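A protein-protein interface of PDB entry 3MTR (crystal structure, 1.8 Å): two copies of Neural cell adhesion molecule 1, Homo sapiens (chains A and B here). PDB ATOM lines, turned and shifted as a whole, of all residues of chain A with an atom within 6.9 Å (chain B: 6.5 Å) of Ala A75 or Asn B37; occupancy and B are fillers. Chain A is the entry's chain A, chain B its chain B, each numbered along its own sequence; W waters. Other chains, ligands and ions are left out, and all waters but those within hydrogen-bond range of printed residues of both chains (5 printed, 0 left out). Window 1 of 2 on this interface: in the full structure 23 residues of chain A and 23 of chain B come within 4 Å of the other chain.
OG1 of Thr A72 sits at hydrogen-bond distance from ND2 of Asn B37. ND2 of Asn B37 is in hydrogen-bond range of OG of Ser A74 (3.5 Å). The side-chain hydroxyl (OH) of Tyr A77 sits at hydrogen-bond distance from the side-chain amide nitrogen (ND2) of Asn B37.
N of Val A42 is in hydrogen-bond range of O of Ser A74, at 3.0 Å. The backbone carbonyl oxygen (O) of Tyr A77 is in hydrogen-bond range of the backbone NH (N) of Tyr A70 (2.8 Å). OG1 of Thr A72 sits at hydrogen-bond distance from O of Ala A75 (2.9 Å). The side-chain carboxylate (OE1) of Glu B79 is in hydrogen-bond range of the side-chain amide nitrogen (NE2) of Gln B35 (3.3 Å). The backbone carbonyl oxygen (O) of Val B36 sits at hydrogen-bond distance from the backbone NH (N) of Val B80 (2.9 Å). N of Tyr B77 sits at hydrogen-bond distance from O of Tyr B70.
Glu B79 touches Thr A72 (OE2 to CG2, 3.5 Å). CG of Pro A73 touches OE1 of Gln B35, 3.0 Å away. O of Gln B35 touches CB of Ser A74 (3.5 Å). Ser A74 touches Val B36 (OG to CA, 3.9 Å). Ala A75 touches Asn B37 (CB to ND2, 3.97 Å). Tyr A77 touches Tyr B77 (CE1 to CE1, 3.4 Å).
Of the printed residues of chain B, Ala A75 touches Asn B37 (3.97 Å). Of chain A, only Thr A72 (3.0 Å), Ser A74 (3.5 Å), Ala A75 (3.97 Å) and Tyr A77 (2.8 Å) come within 4 Å of Asn B37. Of the printed residues of chain B, Ser A74 touches Gln B35 (3.5 Å), Val B36 (3.9 Å) and Asn B37 (3.5 Å). Printed residues of chain A within 4 Å of Glu B79: Thr A72. Of the printed residues of chain A, Val B36 touches Ser A74. Of the printed residues of chain A, Tyr B77 touches Tyr A77 (3.4 Å). Of the printed residues of chain A, Gln B35 touches Pro A73 and Ser A74. Cys A40 touches none of the printed residues of chain B. The nearest printed residue of chain B that does not touch Ala A75 is Gln B35 (7.0 Å). The nearest residue of chain A that does not touch Asn B37 is Pro A73 (5.9 Å). The nearest printed residue of chain A that does not touch Val B36 is Glu A41 (5.6 Å).
Among the printed residues, no Asp or Glu carboxylate lies within 4 Å of a Lys or Arg side-chain nitrogen of the other chain.
Tyr B77 touches its own counterpart, Tyr A77. Of the 9 pairs that touch across the chains among the printed residues, 1 has its exchanged pair printed and touching as well.
Water W4 bridges the side-chain hydroxyl of Tyr B77 and the side-chain hydroxyl of Thr A39. Water W5 lies within hydrogen-bond range of the side-chain hydroxyl (OH) of Tyr A77 and the side-chain hydroxyl (OG1) of Thr B39. Water W3 lies within hydrogen-bond range of OD1 of Asn B37 (2.7 Å), OE1 of Gln B35 (2.7 Å), OG of Ser A74 (2.7 Å) and OG1 of Thr A72 (3.4 Å). Water W1 lies within hydrogen-bond range of OG of Ser A74 (2.8 Å) and N of Asn B37 (2.9 Å). Water W2 lies within hydrogen-bond range of the side-chain hydroxyl (OG1) of Thr B39 (2.8 Å) and the side-chain hydroxyl (OG1) of Thr A39 (2.9 Å).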
ATOM      1  N   THR A  39      17.017  -5.032  -1.409  1.00  0.00           N
ATOM      2  CA  THR A  39      16.359  -4.585  -2.642  1.00  0.00           C
ATOM      3  C   THR A  39      16.279  -3.074  -2.684  1.00  0.00           C
ATOM      4  O   THR A  39      15.757  -2.453  -1.760  1.00  0.00           O
ATOM      5  CB  THR A  39      14.928  -5.153  -2.690  1.00  0.00           C
ATOM      6  OG1 THR A  39      14.975  -6.589  -2.620  1.00  0.00           O
ATOM      7  CG2 THR A  39      14.195  -4.732  -3.970  1.00  0.00           C
ATOM      8  N   CYS A  40      16.764  -2.500  -3.778  1.00  0.00           N
ATOM      9  CA  CYS A  40      16.603  -1.059  -4.002  1.00  0.00           C
ATOM     10  C   CYS A  40      15.885  -0.850  -5.328  1.00  0.00           C
ATOM     11  O   CYS A  40      16.527  -0.890  -6.381  1.00  0.00           O
ATOM     12  CB  CYS A  40      17.968  -0.387  -4.016  1.00  0.00           C
ATOM     13  SG  CYS A  40      17.891   1.402  -4.108  1.00  0.00           S
ATOM     14  N   GLU A  41      14.557  -0.660  -5.269  1.00  0.00           N
ATOM     15  CA  GLU A  41      13.768  -0.425  -6.474  1.00  0.00           C
ATOM     16  C   GLU A  41      13.915   1.033  -6.874  1.00  0.00           C
ATOM     17  O   GLU A  41      13.872   1.898  -6.015  1.00  0.00           O
ATOM     18  CB  GLU A  41      12.282  -0.734  -6.245  1.00  0.00           C
ATOM     19  CG  GLU A  41      12.007  -2.152  -5.789  1.00  0.00           C
ATOM     20  CD  GLU A  41      10.580  -2.309  -5.304  1.00  0.00           C
ATOM     21  OE1 GLU A  41       9.669  -1.890  -6.049  1.00  0.00           O
ATOM     22  OE2 GLU A  41      10.375  -2.838  -4.184  1.00  0.00           O
ATOM     23  N   VAL A  42      14.067   1.309  -8.173  1.00  0.00           N
ATOM     24  CA  VAL A  42      14.371   2.683  -8.580  1.00  0.00           C
ATOM     25  C   VAL A  42      13.415   3.106  -9.688  1.00  0.00           C
ATOM     26  O   VAL A  42      13.124   2.316 -10.589  1.00  0.00           O
ATOM     27  CB  VAL A  42      15.861   2.860  -8.999  1.00  0.00           C
ATOM     28  CG1 VAL A  42      16.241   1.872 -10.036  1.00  0.00           C
ATOM     29  CG2 VAL A  42      16.169   4.283  -9.474  1.00  0.00           C
ATOM     30  N   ILE A  50      23.187   3.660  -9.908  1.00  0.00           N
ATOM     31  CA  ILE A  50      22.947   3.242  -8.517  1.00  0.00           C
ATOM     32  C   ILE A  50      24.280   2.853  -7.920  1.00  0.00           C
ATOM     33  O   ILE A  50      25.047   2.121  -8.545  1.00  0.00           O
ATOM     34  CB  ILE A  50      21.949   2.044  -8.416  1.00  0.00           C
ATOM     35  CG1 ILE A  50      20.503   2.493  -8.701  1.00  0.00           C
ATOM     36  CG2 ILE A  50      21.935   1.503  -7.000  1.00  0.00           C
ATOM     37  CD1 ILE A  50      20.102   2.351 -10.145  1.00  0.00           C
ATOM     38  N   TYR A  70      23.644  -7.080  -8.032  1.00  0.00           N
ATOM     39  CA  TYR A  70      22.916  -7.607  -9.192  1.00  0.00           C
ATOM     40  C   TYR A  70      22.024  -6.484  -9.671  1.00  0.00           C
ATOM     41  O   TYR A  70      21.118  -6.104  -8.953  1.00  0.00           O
ATOM     42  CB  TYR A  70      22.037  -8.795  -8.773  1.00  0.00           C
ATOM     43  CG  TYR A  70      22.805 -10.033  -8.336  1.00  0.00           C
ATOM     44  CD1 TYR A  70      23.415 -10.858  -9.280  1.00  0.00           C
ATOM     45  CD2 TYR A  70      22.899 -10.389  -6.987  1.00  0.00           C
ATOM     46  CE1 TYR A  70      24.114 -11.997  -8.893  1.00  0.00           C
ATOM     47  CE2 TYR A  70      23.599 -11.524  -6.585  1.00  0.00           C
ATOM     48  CZ  TYR A  70      24.198 -12.320  -7.545  1.00  0.00           C
ATOM     49  OH  TYR A  70      24.881 -13.465  -7.170  1.00  0.00           O
ATOM     50  N   ASN A  71      22.294  -5.932 -10.856  1.00  0.00           N
ATOM     51  CA  ASN A  71      21.504  -4.810 -11.374  1.00  0.00           C
ATOM     52  C   ASN A  71      20.492  -5.296 -12.385  1.00  0.00           C
ATOM     53  O   ASN A  71      20.813  -6.096 -13.268  1.00  0.00           O
ATOM     54  CB  ASN A  71      22.400  -3.747 -12.016  1.00  0.00           C
ATOM     55  CG  ASN A  71      23.244  -3.023 -11.000  1.00  0.00           C
ATOM     56  OD1 ASN A  71      24.460  -2.963 -11.132  1.00  0.00           O
ATOM     57  ND2 ASN A  71      22.601  -2.469  -9.973  1.00  0.00           N
ATOM     58  N   THR A  72      19.261  -4.823 -12.238  1.00  0.00           N
ATOM     59  CA  THR A  72      18.231  -5.080 -13.232  1.00  0.00           C
ATOM     60  C   THR A  72      17.663  -3.713 -13.584  1.00  0.00           C
ATOM     61  O   THR A  72      17.900  -2.740 -12.868  1.00  0.00           O
ATOM     62  CB  THR A  72      17.115  -6.028 -12.700  1.00  0.00           C
ATOM     63  OG1 THR A  72      16.315  -5.334 -11.742  1.00  0.00           O
ATOM     64  CG2 THR A  72      17.699  -7.290 -12.057  1.00  0.00           C
ATOM     65  N   PRO A  73      16.943  -3.608 -14.694  1.00  0.00           N
ATOM     66  CA  PRO A  73      16.354  -2.310 -15.075  1.00  0.00           C
ATOM     67  C   PRO A  73      15.490  -1.671 -14.000  1.00  0.00           C
ATOM     68  O   PRO A  73      15.409  -0.455 -13.931  1.00  0.00           O
ATOM     69  CB  PRO A  73      15.512  -2.661 -16.302  1.00  0.00           C
ATOM     70  CG  PRO A  73      16.190  -3.848 -16.871  1.00  0.00           C
ATOM     71  CD  PRO A  73      16.666  -4.650 -15.693  1.00  0.00           C
ATOM     72  N   SER A  74      14.868  -2.451 -13.125  1.00  0.00           N
ATOM     73  CA  SER A  74      13.910  -1.817 -12.215  1.00  0.00           C
ATOM     74  C   SER A  74      14.372  -1.770 -10.766  1.00  0.00           C
ATOM     75  O   SER A  74      13.711  -1.157  -9.919  1.00  0.00           O
ATOM     76  CB  SER A  74      12.530  -2.491 -12.352  1.00  0.00           C
ATOM     77  OG  SER A  74      12.612  -3.843 -11.984  1.00  0.00           O
ATOM     78  N   ALA A  75      15.513  -2.411 -10.480  1.00  0.00           N
ATOM     79  CA  ALA A  75      15.964  -2.552  -9.094  1.00  0.00           C
ATOM     80  C   ALA A  75      17.410  -3.009  -9.058  1.00  0.00           C
ATOM     81  O   ALA A  75      17.844  -3.762  -9.915  1.00  0.00           O
ATOM     82  CB  ALA A  75      15.111  -3.596  -8.345  1.00  0.00           C
ATOM     83  N   SER A  76      18.130  -2.559  -8.041  1.00  0.00           N
ATOM     84  CA  SER A  76      19.482  -3.036  -7.796  1.00  0.00           C
ATOM     85  C   SER A  76      19.412  -3.828  -6.519  1.00  0.00           C
ATOM     86  O   SER A  76      18.702  -3.439  -5.576  1.00  0.00           O
ATOM     87  CB  SER A  76      20.400  -1.826  -7.594  1.00  0.00           C
ATOM     88  OG  SER A  76      21.684  -2.268  -7.238  1.00  0.00           O
ATOM     89  N   TYR A  77      20.133  -4.960  -6.489  1.00  0.00           N
ATOM     90  CA  TYR A  77      20.129  -5.870  -5.366  1.00  0.00           C
ATOM     91  C   TYR A  77      21.555  -5.988  -4.852  1.00  0.00           C
ATOM     92  O   TYR A  77      22.471  -6.314  -5.608  1.00  0.00           O
ATOM     93  CB  TYR A  77      19.645  -7.281  -5.807  1.00  0.00           C
ATOM     94  CG  TYR A  77      18.228  -7.255  -6.331  1.00  0.00           C
ATOM     95  CD1 TYR A  77      17.148  -7.295  -5.454  1.00  0.00           C
ATOM     96  CD2 TYR A  77      17.982  -7.168  -7.698  1.00  0.00           C
ATOM     97  CE1 TYR A  77      15.827  -7.243  -5.929  1.00  0.00           C
ATOM     98  CE2 TYR A  77      16.687  -7.111  -8.189  1.00  0.00           C
ATOM     99  CZ  TYR A  77      15.621  -7.142  -7.309  1.00  0.00           C
ATOM    100  OH  TYR A  77      14.366  -7.090  -7.830  1.00  0.00           O
ATOM    101  N   VAL B  28       2.543  -7.309  -6.575  1.00  0.00           N
ATOM    102  CA  VAL B  28       3.612  -6.600  -7.231  1.00  0.00           C
ATOM    103  C   VAL B  28       2.924  -5.732  -8.276  1.00  0.00           C
ATOM    104  O   VAL B  28       1.993  -6.195  -8.921  1.00  0.00           O
ATOM    105  CB  VAL B  28       4.573  -7.608  -7.901  1.00  0.00           C
ATOM    106  CG1 VAL B  28       5.522  -6.915  -8.715  1.00  0.00           C
ATOM    107  CG2 VAL B  28       5.376  -8.384  -6.818  1.00  0.00           C
ATOM    108  N   GLN B  35       8.902  -2.897 -16.961  1.00  0.00           N
ATOM    109  CA  GLN B  35       9.440  -4.090 -16.283  1.00  0.00           C
ATOM    110  C   GLN B  35       9.326  -3.972 -14.776  1.00  0.00           C
ATOM    111  O   GLN B  35       9.648  -2.930 -14.217  1.00  0.00           O
ATOM    112  CB  GLN B  35      10.921  -4.303 -16.641  1.00  0.00           C
ATOM    113  CG  GLN B  35      11.343  -5.775 -16.396  1.00  0.00           C
ATOM    114  CD  GLN B  35      12.705  -6.102 -16.957  1.00  0.00           C
ATOM    115  OE1 GLN B  35      13.692  -5.470 -16.598  1.00  0.00           O
ATOM    116  NE2 GLN B  35      12.769  -7.105 -17.849  1.00  0.00           N
ATOM    117  N   VAL B  36       8.925  -5.058 -14.113  1.00  0.00           N
ATOM    118  CA  VAL B  36       8.968  -5.115 -12.656  1.00  0.00           C
ATOM    119  C   VAL B  36       9.459  -6.529 -12.321  1.00  0.00           C
ATOM    120  O   VAL B  36       9.296  -7.425 -13.121  1.00  0.00           O
ATOM    121  CB  VAL B  36       7.563  -4.834 -12.040  1.00  0.00           C
ATOM    122  CG1 VAL B  36       6.554  -5.934 -12.372  1.00  0.00           C
ATOM    123  CG2 VAL B  36       7.609  -4.555 -10.543  1.00  0.00           C
ATOM    124  N   ASN B  37      10.077  -6.699 -11.155  1.00  0.00           N
ATOM    125  CA  ASN B  37      10.488  -8.024 -10.718  1.00  0.00           C
ATOM    126  C   ASN B  37       9.524  -8.577  -9.664  1.00  0.00           C
ATOM    127  O   ASN B  37       9.127  -7.873  -8.719  1.00  0.00           O
ATOM    128  CB  ASN B  37      11.910  -7.964 -10.142  1.00  0.00           C
ATOM    129  CG  ASN B  37      12.876  -7.316 -11.086  1.00  0.00           C
ATOM    130  OD1 ASN B  37      12.686  -7.371 -12.315  1.00  0.00           O
ATOM    131  ND2 ASN B  37      13.928  -6.684 -10.534  1.00  0.00           N
ATOM    132  N   ILE B  38       9.142  -9.837  -9.826  1.00  0.00           N
ATOM    133  CA  ILE B  38       8.375 -10.531  -8.797  1.00  0.00           C
ATOM    134  C   ILE B  38       9.416 -11.344  -8.008  1.00  0.00           C
ATOM    135  O   ILE B  38      10.188 -12.056  -8.603  1.00  0.00           O
ATOM    136  CB  ILE B  38       7.340 -11.476  -9.405  1.00  0.00           C
ATOM    137  CG1 ILE B  38       6.434 -10.731 -10.401  1.00  0.00           C
ATOM    138  CG2 ILE B  38       6.499 -12.108  -8.305  1.00  0.00           C
ATOM    139  CD1 ILE B  38       5.372 -11.582 -11.051  1.00  0.00           C
ATOM    140  N   THR B  39       9.434 -11.205  -6.690  1.00  0.00           N
ATOM    141  CA  THR B  39      10.477 -11.814  -5.877  1.00  0.00           C
ATOM    142  C   THR B  39       9.978 -13.089  -5.212  1.00  0.00           C
ATOM    143  O   THR B  39       8.969 -13.085  -4.534  1.00  0.00           O
ATOM    144  CB  THR B  39      10.846 -10.875  -4.767  1.00  0.00           C
ATOM    145  OG1 THR B  39      11.282  -9.627  -5.331  1.00  0.00           O
ATOM    146  CG2 THR B  39      11.937 -11.452  -3.876  1.00  0.00           C
ATOM    147  N   TYR B  70      15.621 -14.022 -13.499  1.00  0.00           N
ATOM    148  CA  TYR B  70      16.925 -13.669 -12.944  1.00  0.00           C
ATOM    149  C   TYR B  70      17.089 -14.438 -11.626  1.00  0.00           C
ATOM    150  O   TYR B  70      16.376 -14.155 -10.666  1.00  0.00           O
ATOM    151  CB  TYR B  70      17.013 -12.152 -12.714  1.00  0.00           C
ATOM    152  N   TYR B  77      13.971 -13.998  -9.353  1.00  0.00           N
ATOM    153  CA  TYR B  77      13.160 -12.842  -9.733  1.00  0.00           C
ATOM    154  C   TYR B  77      12.588 -13.046 -11.134  1.00  0.00           C
ATOM    155  O   TYR B  77      13.320 -13.367 -12.086  1.00  0.00           O
ATOM    156  CB  TYR B  77      13.978 -11.538  -9.673  1.00  0.00           C
ATOM    157  CG  TYR B  77      14.611 -11.290  -8.321  1.00  0.00           C
ATOM    158  CD1 TYR B  77      13.925 -10.599  -7.318  1.00  0.00           C
ATOM    159  CD2 TYR B  77      15.883 -11.760  -8.038  1.00  0.00           C
ATOM    160  CE1 TYR B  77      14.533 -10.386  -6.051  1.00  0.00           C
ATOM    161  CE2 TYR B  77      16.485 -11.555  -6.779  1.00  0.00           C
ATOM    162  CZ  TYR B  77      15.806 -10.867  -5.811  1.00  0.00           C
ATOM    163  OH  TYR B  77      16.403 -10.689  -4.572  1.00  0.00           O
ATOM    164  N   LEU B  78      11.291 -12.839 -11.252  1.00  0.00           N
ATOM    165  CA  LEU B  78      10.631 -12.946 -12.542  1.00  0.00           C
ATOM    166  C   LEU B  78      10.458 -11.532 -13.002  1.00  0.00           C
ATOM    167  O   LEU B  78       9.744 -10.770 -12.341  1.00  0.00           O
ATOM    168  CB  LEU B  78       9.264 -13.613 -12.412  1.00  0.00           C
ATOM    169  CG  LEU B  78       8.623 -14.019 -13.729  1.00  0.00           C
ATOM    170  CD1 LEU B  78       9.459 -15.143 -14.395  1.00  0.00           C
ATOM    171  CD2 LEU B  78       7.153 -14.465 -13.494  1.00  0.00           C
ATOM    172  N   GLU B  79      11.141 -11.206 -14.092  1.00  0.00           N
ATOM    173  CA  GLU B  79      11.117  -9.867 -14.689  1.00  0.00           C
ATOM    174  C   GLU B  79       9.989  -9.889 -15.713  1.00  0.00           C
ATOM    175  O   GLU B  79      10.130 -10.546 -16.748  1.00  0.00           O
ATOM    176  CB  GLU B  79      12.456  -9.573 -15.397  1.00  0.00           C
ATOM    177  CG  GLU B  79      13.748  -9.670 -14.514  1.00  0.00           C
ATOM    178  CD  GLU B  79      15.045  -9.233 -15.223  1.00  0.00           C
ATOM    179  OE1 GLU B  79      15.077  -9.044 -16.466  1.00  0.00           O
ATOM    180  OE2 GLU B  79      16.074  -9.086 -14.537  1.00  0.00           O
ATOM    181  N   VAL B  80       8.882  -9.197 -15.435  1.00  0.00           N
ATOM    182  CA  VAL B  80       7.731  -9.156 -16.360  1.00  0.00           C
ATOM    183  C   VAL B  80       7.549  -7.763 -16.909  1.00  0.00           C
ATOM    184  O   VAL B  80       7.547  -6.800 -16.147  1.00  0.00           O
ATOM    185  CB  VAL B  80       6.366  -9.570 -15.656  1.00  0.00           C
ATOM    186  CG1 VAL B  80       5.229  -9.647 -16.650  1.00  0.00           C
ATOM    187  CG2 VAL B  80       6.501 -10.933 -14.944  1.00  0.00           C
HETATM  188  O   HOH W   1      11.115  -4.392  -9.667  1.00  0.00           O
HETATM  189  O   HOH W   2      12.571  -7.920  -3.490  1.00  0.00           O
HETATM  190  O   HOH W   3      13.673  -5.433 -13.899  1.00  0.00           O
HETATM  191  O   HOH W   4      14.966  -9.135  -3.134  1.00  0.00           O
HETATM  192  O   HOH W   5      12.405  -7.216  -6.180  1.00  0.00           O
